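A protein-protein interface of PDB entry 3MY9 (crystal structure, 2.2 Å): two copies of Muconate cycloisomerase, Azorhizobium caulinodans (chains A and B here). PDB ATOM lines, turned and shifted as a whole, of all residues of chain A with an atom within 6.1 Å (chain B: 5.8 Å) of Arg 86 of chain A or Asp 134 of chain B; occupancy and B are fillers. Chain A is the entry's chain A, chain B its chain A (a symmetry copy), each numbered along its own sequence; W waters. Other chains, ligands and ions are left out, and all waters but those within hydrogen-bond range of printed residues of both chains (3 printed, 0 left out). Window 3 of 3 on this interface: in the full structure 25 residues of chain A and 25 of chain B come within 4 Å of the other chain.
Of the 10 printed residues of chain A, 4 touch a printed residue of chain B. Of the 12 printed residues of chain B, 4 touch a printed residue of chain A. Along chain B the printed residues that touch a printed residue of chain A span positions 129 to 134. Among the printed residues, 5 pairs touch across the chains.
Water W2 lies within hydrogen-bond range of O of Gly 130 of chain B (2.6 Å), NE of Arg 88 of chain A (2.7 Å) and O of Gly 129 of chain B (3.4 Å). Water W3 lies within hydrogen-bond range of the side-chain carboxylate (OD2) of Asp 134 of chain B (2.7 Å) and the guanidinium group (NH2) of Arg 86 of chain A (3.2 Å). Water W1 bridges N of Arg 131 of chain B (3.1 Å) and O of Lys 85 of chain A (3.4 Å).
Gly 130 of chain B touches Lys 85 of chain A (CA to O, 3.3 Å). Arg 131 of chain B touches Arg 86 of chain A. Gly 129 of chain B touches Val 87 of chain A (O to N, 3.9 Å).
The backbone NH (N) of Arg 88 of chain A sits at hydrogen-bond distance from the backbone carbonyl oxygen (O) of Gly 129 of chain B (3.4 Å). The side-chain carboxylate (OD1) of Asp 134 of chain B lies within salt-bridge range of the guanidinium group (NH1) of Arg 86 of chain A, at 2.7 Å.
The backbone carbonyl oxygen of Asp 134 of chain B is in hydrogen-bond range of the backbone NH of Val 352 of chain B, 3.1 Å away. OE1 of Glu 89 of chain A is in salt-bridge range of NH2 of Arg 86 of chain A (3.1 Å). O of Val 352 of chain B lies within hydrogen-bond range of NH2 of Arg 131 of chain B (3.1 Å). NH1 of Arg 131 of chain B is in salt-bridge range of OD1 of Asp 134 of chain B.
No position is printed for both chains. Of the 5 pairs that touch across the chains among the printed residues, none has its exchanged pair printed and touching as well.
Arg 86 of chain A touches just these residues of chain B: Arg 131 and Asp 134. Asp 134 of chain B touches just one residue of chain A: Arg 86 (2.7 Å). Of the printed residues of chain B, Arg 88 of chain A touches Gly 129 (3.4 Å). Printed residues of chain B within 4 Å of Val 87 of chain A: Gly 129. Of the printed residues of chain B, Lys 85 of chain A touches Gly 130 (3.3 Å). Of the printed residues of chain A, Gly 130 of chain B touches Lys 85 (3.3 Å). Glu 89 of chain A touches none of the printed residues of chain B. The nearest residue of chain B that does not touch Arg 86 of chain A is Val 132 of chain B (4.3 Å). The nearest printed residue of chain A that does not touch Asp 134 of chain B is Glu 89 of chain A (6.5 Å). The nearest printed residue of chain B that does not touch Val 87 of chain A is Gly 130 of chain B (5.1 Å).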
ATOM      1  N   PRO A  83      24.440  11.207  -9.159  1.00  0.00           N
ATOM      2  CA  PRO A  83      23.120  11.256  -8.503  1.00  0.00           C
ATOM      3  C   PRO A  83      21.970  11.099  -9.495  1.00  0.00           C
ATOM      4  O   PRO A  83      21.859  11.867 -10.445  1.00  0.00           O
ATOM      5  CB  PRO A  83      23.103  12.628  -7.804  1.00  0.00           C
ATOM      6  CG  PRO A  83      24.539  13.186  -7.941  1.00  0.00           C
ATOM      7  CD  PRO A  83      25.122  12.516  -9.143  1.00  0.00           C
ATOM      8  N   ILE A  84      21.118  10.103  -9.258  1.00  0.00           N
ATOM      9  CA  ILE A  84      20.102   9.687 -10.224  1.00  0.00           C
ATOM     10  C   ILE A  84      19.019  10.747 -10.456  1.00  0.00           C
ATOM     11  O   ILE A  84      18.435  10.770 -11.513  1.00  0.00           O
ATOM     12  CB  ILE A  84      19.451   8.336  -9.808  1.00  0.00           C
ATOM     13  CG1 ILE A  84      20.499   7.221  -9.830  1.00  0.00           C
ATOM     14  CG2 ILE A  84      18.308   7.948 -10.747  1.00  0.00           C
ATOM     15  CD1 ILE A  84      20.089   6.005  -9.016  1.00  0.00           C
ATOM     16  N   LYS A  85      18.753  11.599  -9.466  1.00  0.00           N
ATOM     17  CA  LYS A  85      17.869  12.764  -9.631  1.00  0.00           C
ATOM     18  C   LYS A  85      18.459  13.835 -10.541  1.00  0.00           C
ATOM     19  O   LYS A  85      17.729  14.733 -10.942  1.00  0.00           O
ATOM     20  CB  LYS A  85      17.604  13.472  -8.294  1.00  0.00           C
ATOM     21  CG  LYS A  85      16.730  12.783  -7.279  1.00  0.00           C
ATOM     22  CD  LYS A  85      17.030  13.337  -5.830  1.00  0.00           C
ATOM     23  CE  LYS A  85      16.106  14.495  -5.443  1.00  0.00           C
ATOM     24  NZ  LYS A  85      16.038  14.818  -4.014  1.00  0.00           N
ATOM     25  N   ARG A  86      19.752  13.788 -10.863  1.00  0.00           N
ATOM     26  CA  ARG A  86      20.361  14.841 -11.715  1.00  0.00           C
ATOM     27  C   ARG A  86      20.704  14.361 -13.113  1.00  0.00           C
ATOM     28  O   ARG A  86      21.855  14.413 -13.532  1.00  0.00           O
ATOM     29  CB  ARG A  86      21.608  15.436 -11.068  1.00  0.00           C
ATOM     30  CG  ARG A  86      21.326  16.094  -9.754  1.00  0.00           C
ATOM     31  CD  ARG A  86      22.521  16.946  -9.285  1.00  0.00           C
ATOM     32  NE  ARG A  86      22.202  17.614  -8.035  1.00  0.00           N
ATOM     33  CZ  ARG A  86      22.664  18.806  -7.666  1.00  0.00           C
ATOM     34  NH1 ARG A  86      22.285  19.303  -6.502  1.00  0.00           N
ATOM     35  NH2 ARG A  86      23.509  19.506  -8.442  1.00  0.00           N
ATOM     36  N   VAL A  87      19.679  13.961 -13.847  1.00  0.00           N
ATOM     37  CA  VAL A  87      19.835  13.424 -15.185  1.00  0.00           C
ATOM     38  C   VAL A  87      20.406  14.441 -16.200  1.00  0.00           C
ATOM     39  O   VAL A  87      21.350  14.135 -16.934  1.00  0.00           O
ATOM     40  CB  VAL A  87      18.486  12.882 -15.679  1.00  0.00           C
ATOM     41  CG1 VAL A  87      18.632  12.262 -17.054  1.00  0.00           C
ATOM     42  CG2 VAL A  87      17.938  11.851 -14.632  1.00  0.00           C
ATOM     43  N   ARG A  88      19.837  15.647 -16.235  1.00  0.00           N
ATOM     44  CA  ARG A  88      20.312  16.674 -17.156  1.00  0.00           C
ATOM     45  C   ARG A  88      21.750  17.046 -16.857  1.00  0.00           C
ATOM     46  O   ARG A  88      22.511  17.338 -17.774  1.00  0.00           O
ATOM     47  CB  ARG A  88      19.437  17.932 -17.139  1.00  0.00           C
ATOM     48  CG  ARG A  88      19.503  18.707 -18.473  1.00  0.00           C
ATOM     49  CD  ARG A  88      18.806  20.065 -18.408  1.00  0.00           C
ATOM     50  NE  ARG A  88      17.413  20.010 -17.928  1.00  0.00           N
ATOM     51  CZ  ARG A  88      16.350  19.881 -18.700  1.00  0.00           C
ATOM     52  NH1 ARG A  88      16.486  19.733 -20.003  1.00  0.00           N
ATOM     53  NH2 ARG A  88      15.135  19.873 -18.162  1.00  0.00           N
ATOM     54  N   GLU A  89      22.118  17.050 -15.576  1.00  0.00           N
ATOM     55  CA  GLU A  89      23.487  17.363 -15.170  1.00  0.00           C
ATOM     56  C   GLU A  89      24.458  16.303 -15.685  1.00  0.00           C
ATOM     57  O   GLU A  89      25.558  16.632 -16.122  1.00  0.00           O
ATOM     58  CB  GLU A  89      23.607  17.461 -13.646  1.00  0.00           C
ATOM     59  CG  GLU A  89      25.002  17.886 -13.151  1.00  0.00           C
ATOM     60  CD  GLU A  89      25.121  17.850 -11.630  1.00  0.00           C
ATOM     61  OE1 GLU A  89      25.227  18.927 -10.998  1.00  0.00           O
ATOM     62  OE2 GLU A  89      25.103  16.735 -11.062  1.00  0.00           O
ATOM     63  N   LEU A  90      24.073  15.029 -15.580  1.00  0.00           N
ATOM     64  CA  LEU A  90      24.926  13.933 -16.063  1.00  0.00           C
ATOM     65  C   LEU A  90      25.031  13.995 -17.584  1.00  0.00           C
ATOM     66  O   LEU A  90      26.110  13.776 -18.106  1.00  0.00           O
ATOM     67  CB  LEU A  90      24.406  12.546 -15.633  1.00  0.00           C
ATOM     68  CG  LEU A  90      25.281  11.328 -16.031  1.00  0.00           C
ATOM     69  CD1 LEU A  90      26.588  11.334 -15.262  1.00  0.00           C
ATOM     70  CD2 LEU A  90      24.551   9.978 -15.811  1.00  0.00           C
ATOM     71  N   MET A  91      23.929  14.289 -18.286  1.00  0.00           N
ATOM     72  CA  MET A  91      23.969  14.381 -19.763  1.00  0.00           C
ATOM     73  C   MET A  91      24.921  15.471 -20.232  1.00  0.00           C
ATOM     74  O   MET A  91      25.585  15.306 -21.262  1.00  0.00           O
ATOM     75  CB  MET A  91      22.575  14.621 -20.376  1.00  0.00           C
ATOM     76  CG  MET A  91      22.572  14.761 -21.942  1.00  0.00           C
ATOM     77  SD  MET A  91      23.155  13.316 -22.923  1.00  0.00           S
ATOM     78  CE  MET A  91      21.741  12.202 -22.657  1.00  0.00           C
ATOM     79  N   LEU A 112      18.383   5.850 -16.048  1.00  0.00           N
ATOM     80  CA  LEU A 112      18.289   6.687 -14.834  1.00  0.00           C
ATOM     81  C   LEU A 112      16.862   7.156 -14.608  1.00  0.00           C
ATOM     82  O   LEU A 112      16.423   7.254 -13.464  1.00  0.00           O
ATOM     83  CB  LEU A 112      19.201   7.920 -14.914  1.00  0.00           C
ATOM     84  CG  LEU A 112      20.592   7.787 -14.322  1.00  0.00           C
ATOM     85  CD1 LEU A 112      21.279   6.520 -14.780  1.00  0.00           C
ATOM     86  CD2 LEU A 112      21.377   9.032 -14.724  1.00  0.00           C
ATOM     87  N   GLY B 129      13.825  18.071 -14.577  1.00  0.00           N
ATOM     88  CA  GLY B 129      15.035  17.510 -15.160  1.00  0.00           C
ATOM     89  C   GLY B 129      16.161  17.365 -14.165  1.00  0.00           C
ATOM     90  O   GLY B 129      17.222  16.852 -14.512  1.00  0.00           O
ATOM     91  N   GLY B 130      15.933  17.835 -12.942  1.00  0.00           N
ATOM     92  CA  GLY B 130      16.910  17.773 -11.883  1.00  0.00           C
ATOM     93  C   GLY B 130      17.686  19.069 -11.735  1.00  0.00           C
ATOM     94  O   GLY B 130      17.845  19.816 -12.692  1.00  0.00           O
ATOM     95  N   ARG B 131      18.144  19.328 -10.516  1.00  0.00           N
ATOM     96  CA  ARG B 131      19.045  20.432 -10.231  1.00  0.00           C
ATOM     97  C   ARG B 131      20.326  20.328 -11.032  1.00  0.00           C
ATOM     98  O   ARG B 131      20.871  19.240 -11.216  1.00  0.00           O
ATOM     99  CB  ARG B 131      19.481  20.453  -8.770  1.00  0.00           C
ATOM    100  CG  ARG B 131      18.403  20.752  -7.748  1.00  0.00           C
ATOM    101  CD  ARG B 131      19.051  21.102  -6.390  1.00  0.00           C
ATOM    102  NE  ARG B 131      18.058  21.526  -5.395  1.00  0.00           N
ATOM    103  CZ  ARG B 131      18.375  22.005  -4.192  1.00  0.00           C
ATOM    104  NH1 ARG B 131      19.652  22.104  -3.828  1.00  0.00           N
ATOM    105  NH2 ARG B 131      17.423  22.393  -3.347  1.00  0.00           N
ATOM    106  N   VAL B 132      20.783  21.498 -11.475  1.00  0.00           N
ATOM    107  CA  VAL B 132      22.069  21.688 -12.066  1.00  0.00           C
ATOM    108  C   VAL B 132      22.889  22.688 -11.239  1.00  0.00           C
ATOM    109  O   VAL B 132      24.087  22.826 -11.447  1.00  0.00           O
ATOM    110  CB  VAL B 132      21.896  22.173 -13.511  1.00  0.00           C
ATOM    111  CG1 VAL B 132      23.177  22.715 -14.016  1.00  0.00           C
ATOM    112  CG2 VAL B 132      21.400  20.975 -14.385  1.00  0.00           C
ATOM    113  N   ARG B 133      22.236  23.349 -10.280  1.00  0.00           N
ATOM    114  CA  ARG B 133      22.915  24.194  -9.304  1.00  0.00           C
ATOM    115  C   ARG B 133      22.138  24.253  -7.995  1.00  0.00           C
ATOM    116  O   ARG B 133      20.934  24.015  -7.964  1.00  0.00           O
ATOM    117  CB  ARG B 133      23.115  25.610  -9.882  1.00  0.00           C
ATOM    118  CG  ARG B 133      21.820  26.283 -10.328  1.00  0.00           C
ATOM    119  CD  ARG B 133      22.092  27.678 -10.846  1.00  0.00           C
ATOM    120  NE  ARG B 133      22.848  27.703 -12.094  1.00  0.00           N
ATOM    121  CZ  ARG B 133      22.331  27.573 -13.314  1.00  0.00           C
ATOM    122  NH1 ARG B 133      21.020  27.410 -13.507  1.00  0.00           N
ATOM    123  NH2 ARG B 133      23.134  27.642 -14.364  1.00  0.00           N
ATOM    124  N   ASP B 134      22.847  24.589  -6.919  1.00  0.00           N
ATOM    125  CA  ASP B 134      22.286  24.625  -5.566  1.00  0.00           C
ATOM    126  C   ASP B 134      22.108  26.024  -4.963  1.00  0.00           C
ATOM    127  O   ASP B 134      21.453  26.180  -3.917  1.00  0.00           O
ATOM    128  CB  ASP B 134      23.206  23.829  -4.653  1.00  0.00           C
ATOM    129  CG  ASP B 134      23.380  22.395  -5.119  1.00  0.00           C
ATOM    130  OD1 ASP B 134      22.364  21.711  -5.377  1.00  0.00           O
ATOM    131  OD2 ASP B 134      24.548  21.968  -5.240  1.00  0.00           O
ATOM    132  N   ARG B 135      22.748  27.012  -5.603  1.00  0.00           N
ATOM    133  CA  ARG B 135      22.690  28.417  -5.231  1.00  0.00           C
ATOM    134  C   ARG B 135      22.492  29.229  -6.514  1.00  0.00           C
ATOM    135  O   ARG B 135      22.852  28.766  -7.599  1.00  0.00           O
ATOM    136  CB  ARG B 135      24.019  28.851  -4.588  1.00  0.00           C
ATOM    137  CG  ARG B 135      24.505  27.983  -3.491  1.00  0.00           C
ATOM    138  CD  ARG B 135      25.897  28.359  -3.027  1.00  0.00           C
ATOM    139  NE  ARG B 135      26.254  27.656  -1.803  1.00  0.00           N
ATOM    140  CZ  ARG B 135      27.311  27.957  -1.044  1.00  0.00           C
ATOM    141  NH1 ARG B 135      28.136  28.950  -1.386  1.00  0.00           N
ATOM    142  NH2 ARG B 135      27.554  27.267   0.053  1.00  0.00           N
ATOM    143  N   ILE B 136      21.941  30.433  -6.401  1.00  0.00           N
ATOM    144  CA  ILE B 136      21.739  31.293  -7.543  1.00  0.00           C
ATOM    145  C   ILE B 136      22.347  32.663  -7.247  1.00  0.00           C
ATOM    146  O   ILE B 136      21.926  33.319  -6.304  1.00  0.00           O
ATOM    147  CB  ILE B 136      20.265  31.511  -7.860  1.00  0.00           C
ATOM    148  CG1 ILE B 136      19.504  30.179  -7.927  1.00  0.00           C
ATOM    149  CG2 ILE B 136      20.147  32.270  -9.190  1.00  0.00           C
ATOM    150  CD1 ILE B 136      17.996  30.337  -8.020  1.00  0.00           C
ATOM    151  N   ALA B 316      17.199  26.634 -10.575  1.00  0.00           N
ATOM    152  CA  ALA B 316      18.004  25.515 -10.121  1.00  0.00           C
ATOM    153  C   ALA B 316      18.104  24.396 -11.175  1.00  0.00           C
ATOM    154  O   ALA B 316      19.133  23.709 -11.267  1.00  0.00           O
ATOM    155  CB  ALA B 316      17.422  24.975  -8.822  1.00  0.00           C
ATOM    156  N   VAL B 350      21.178  33.242  -3.559  1.00  0.00           N
ATOM    157  CA  VAL B 350      20.006  32.612  -2.963  1.00  0.00           C
ATOM    158  C   VAL B 350      20.294  31.123  -2.735  1.00  0.00           C
ATOM    159  O   VAL B 350      20.896  30.473  -3.584  1.00  0.00           O
ATOM    160  CB  VAL B 350      18.769  32.730  -3.911  1.00  0.00           C
ATOM    161  CG1 VAL B 350      17.597  31.934  -3.370  1.00  0.00           C
ATOM    162  CG2 VAL B 350      18.382  34.176  -4.102  1.00  0.00           C
ATOM    163  N   ILE B 351      19.862  30.582  -1.601  1.00  0.00           N
ATOM    164  CA  ILE B 351      20.037  29.155  -1.311  1.00  0.00           C
ATOM    165  C   ILE B 351      18.783  28.483  -1.809  1.00  0.00           C
ATOM    166  O   ILE B 351      17.679  28.908  -1.447  1.00  0.00           O
ATOM    167  CB  ILE B 351      20.228  28.884   0.168  1.00  0.00           C
ATOM    168  CG1 ILE B 351      21.268  29.837   0.746  1.00  0.00           C
ATOM    169  CG2 ILE B 351      20.661  27.412   0.401  1.00  0.00           C
ATOM    170  CD1 ILE B 351      22.609  29.668   0.118  1.00  0.00           C
ATOM    171  N   VAL B 352      18.938  27.505  -2.706  1.00  0.00           N
ATOM    172  CA  VAL B 352      17.771  26.834  -3.281  1.00  0.00           C
ATOM    173  C   VAL B 352      17.224  25.932  -2.188  1.00  0.00           C
ATOM    174  O   VAL B 352      17.934  25.035  -1.715  1.00  0.00           O
ATOM    175  CB  VAL B 352      18.093  26.035  -4.591  1.00  0.00           C
ATOM    176  CG1 VAL B 352      16.850  25.319  -5.108  1.00  0.00           C
ATOM    177  CG2 VAL B 352      18.621  26.959  -5.685  1.00  0.00           C
HETATM  178  O   HOH W   1      17.839  17.004  -8.462  1.00  0.00           O
HETATM  179  O   HOH W   2      17.336  20.175 -15.238  1.00  0.00           O
HETATM  180  O   HOH W   3      25.613  21.772  -7.672  1.00  0.00           O
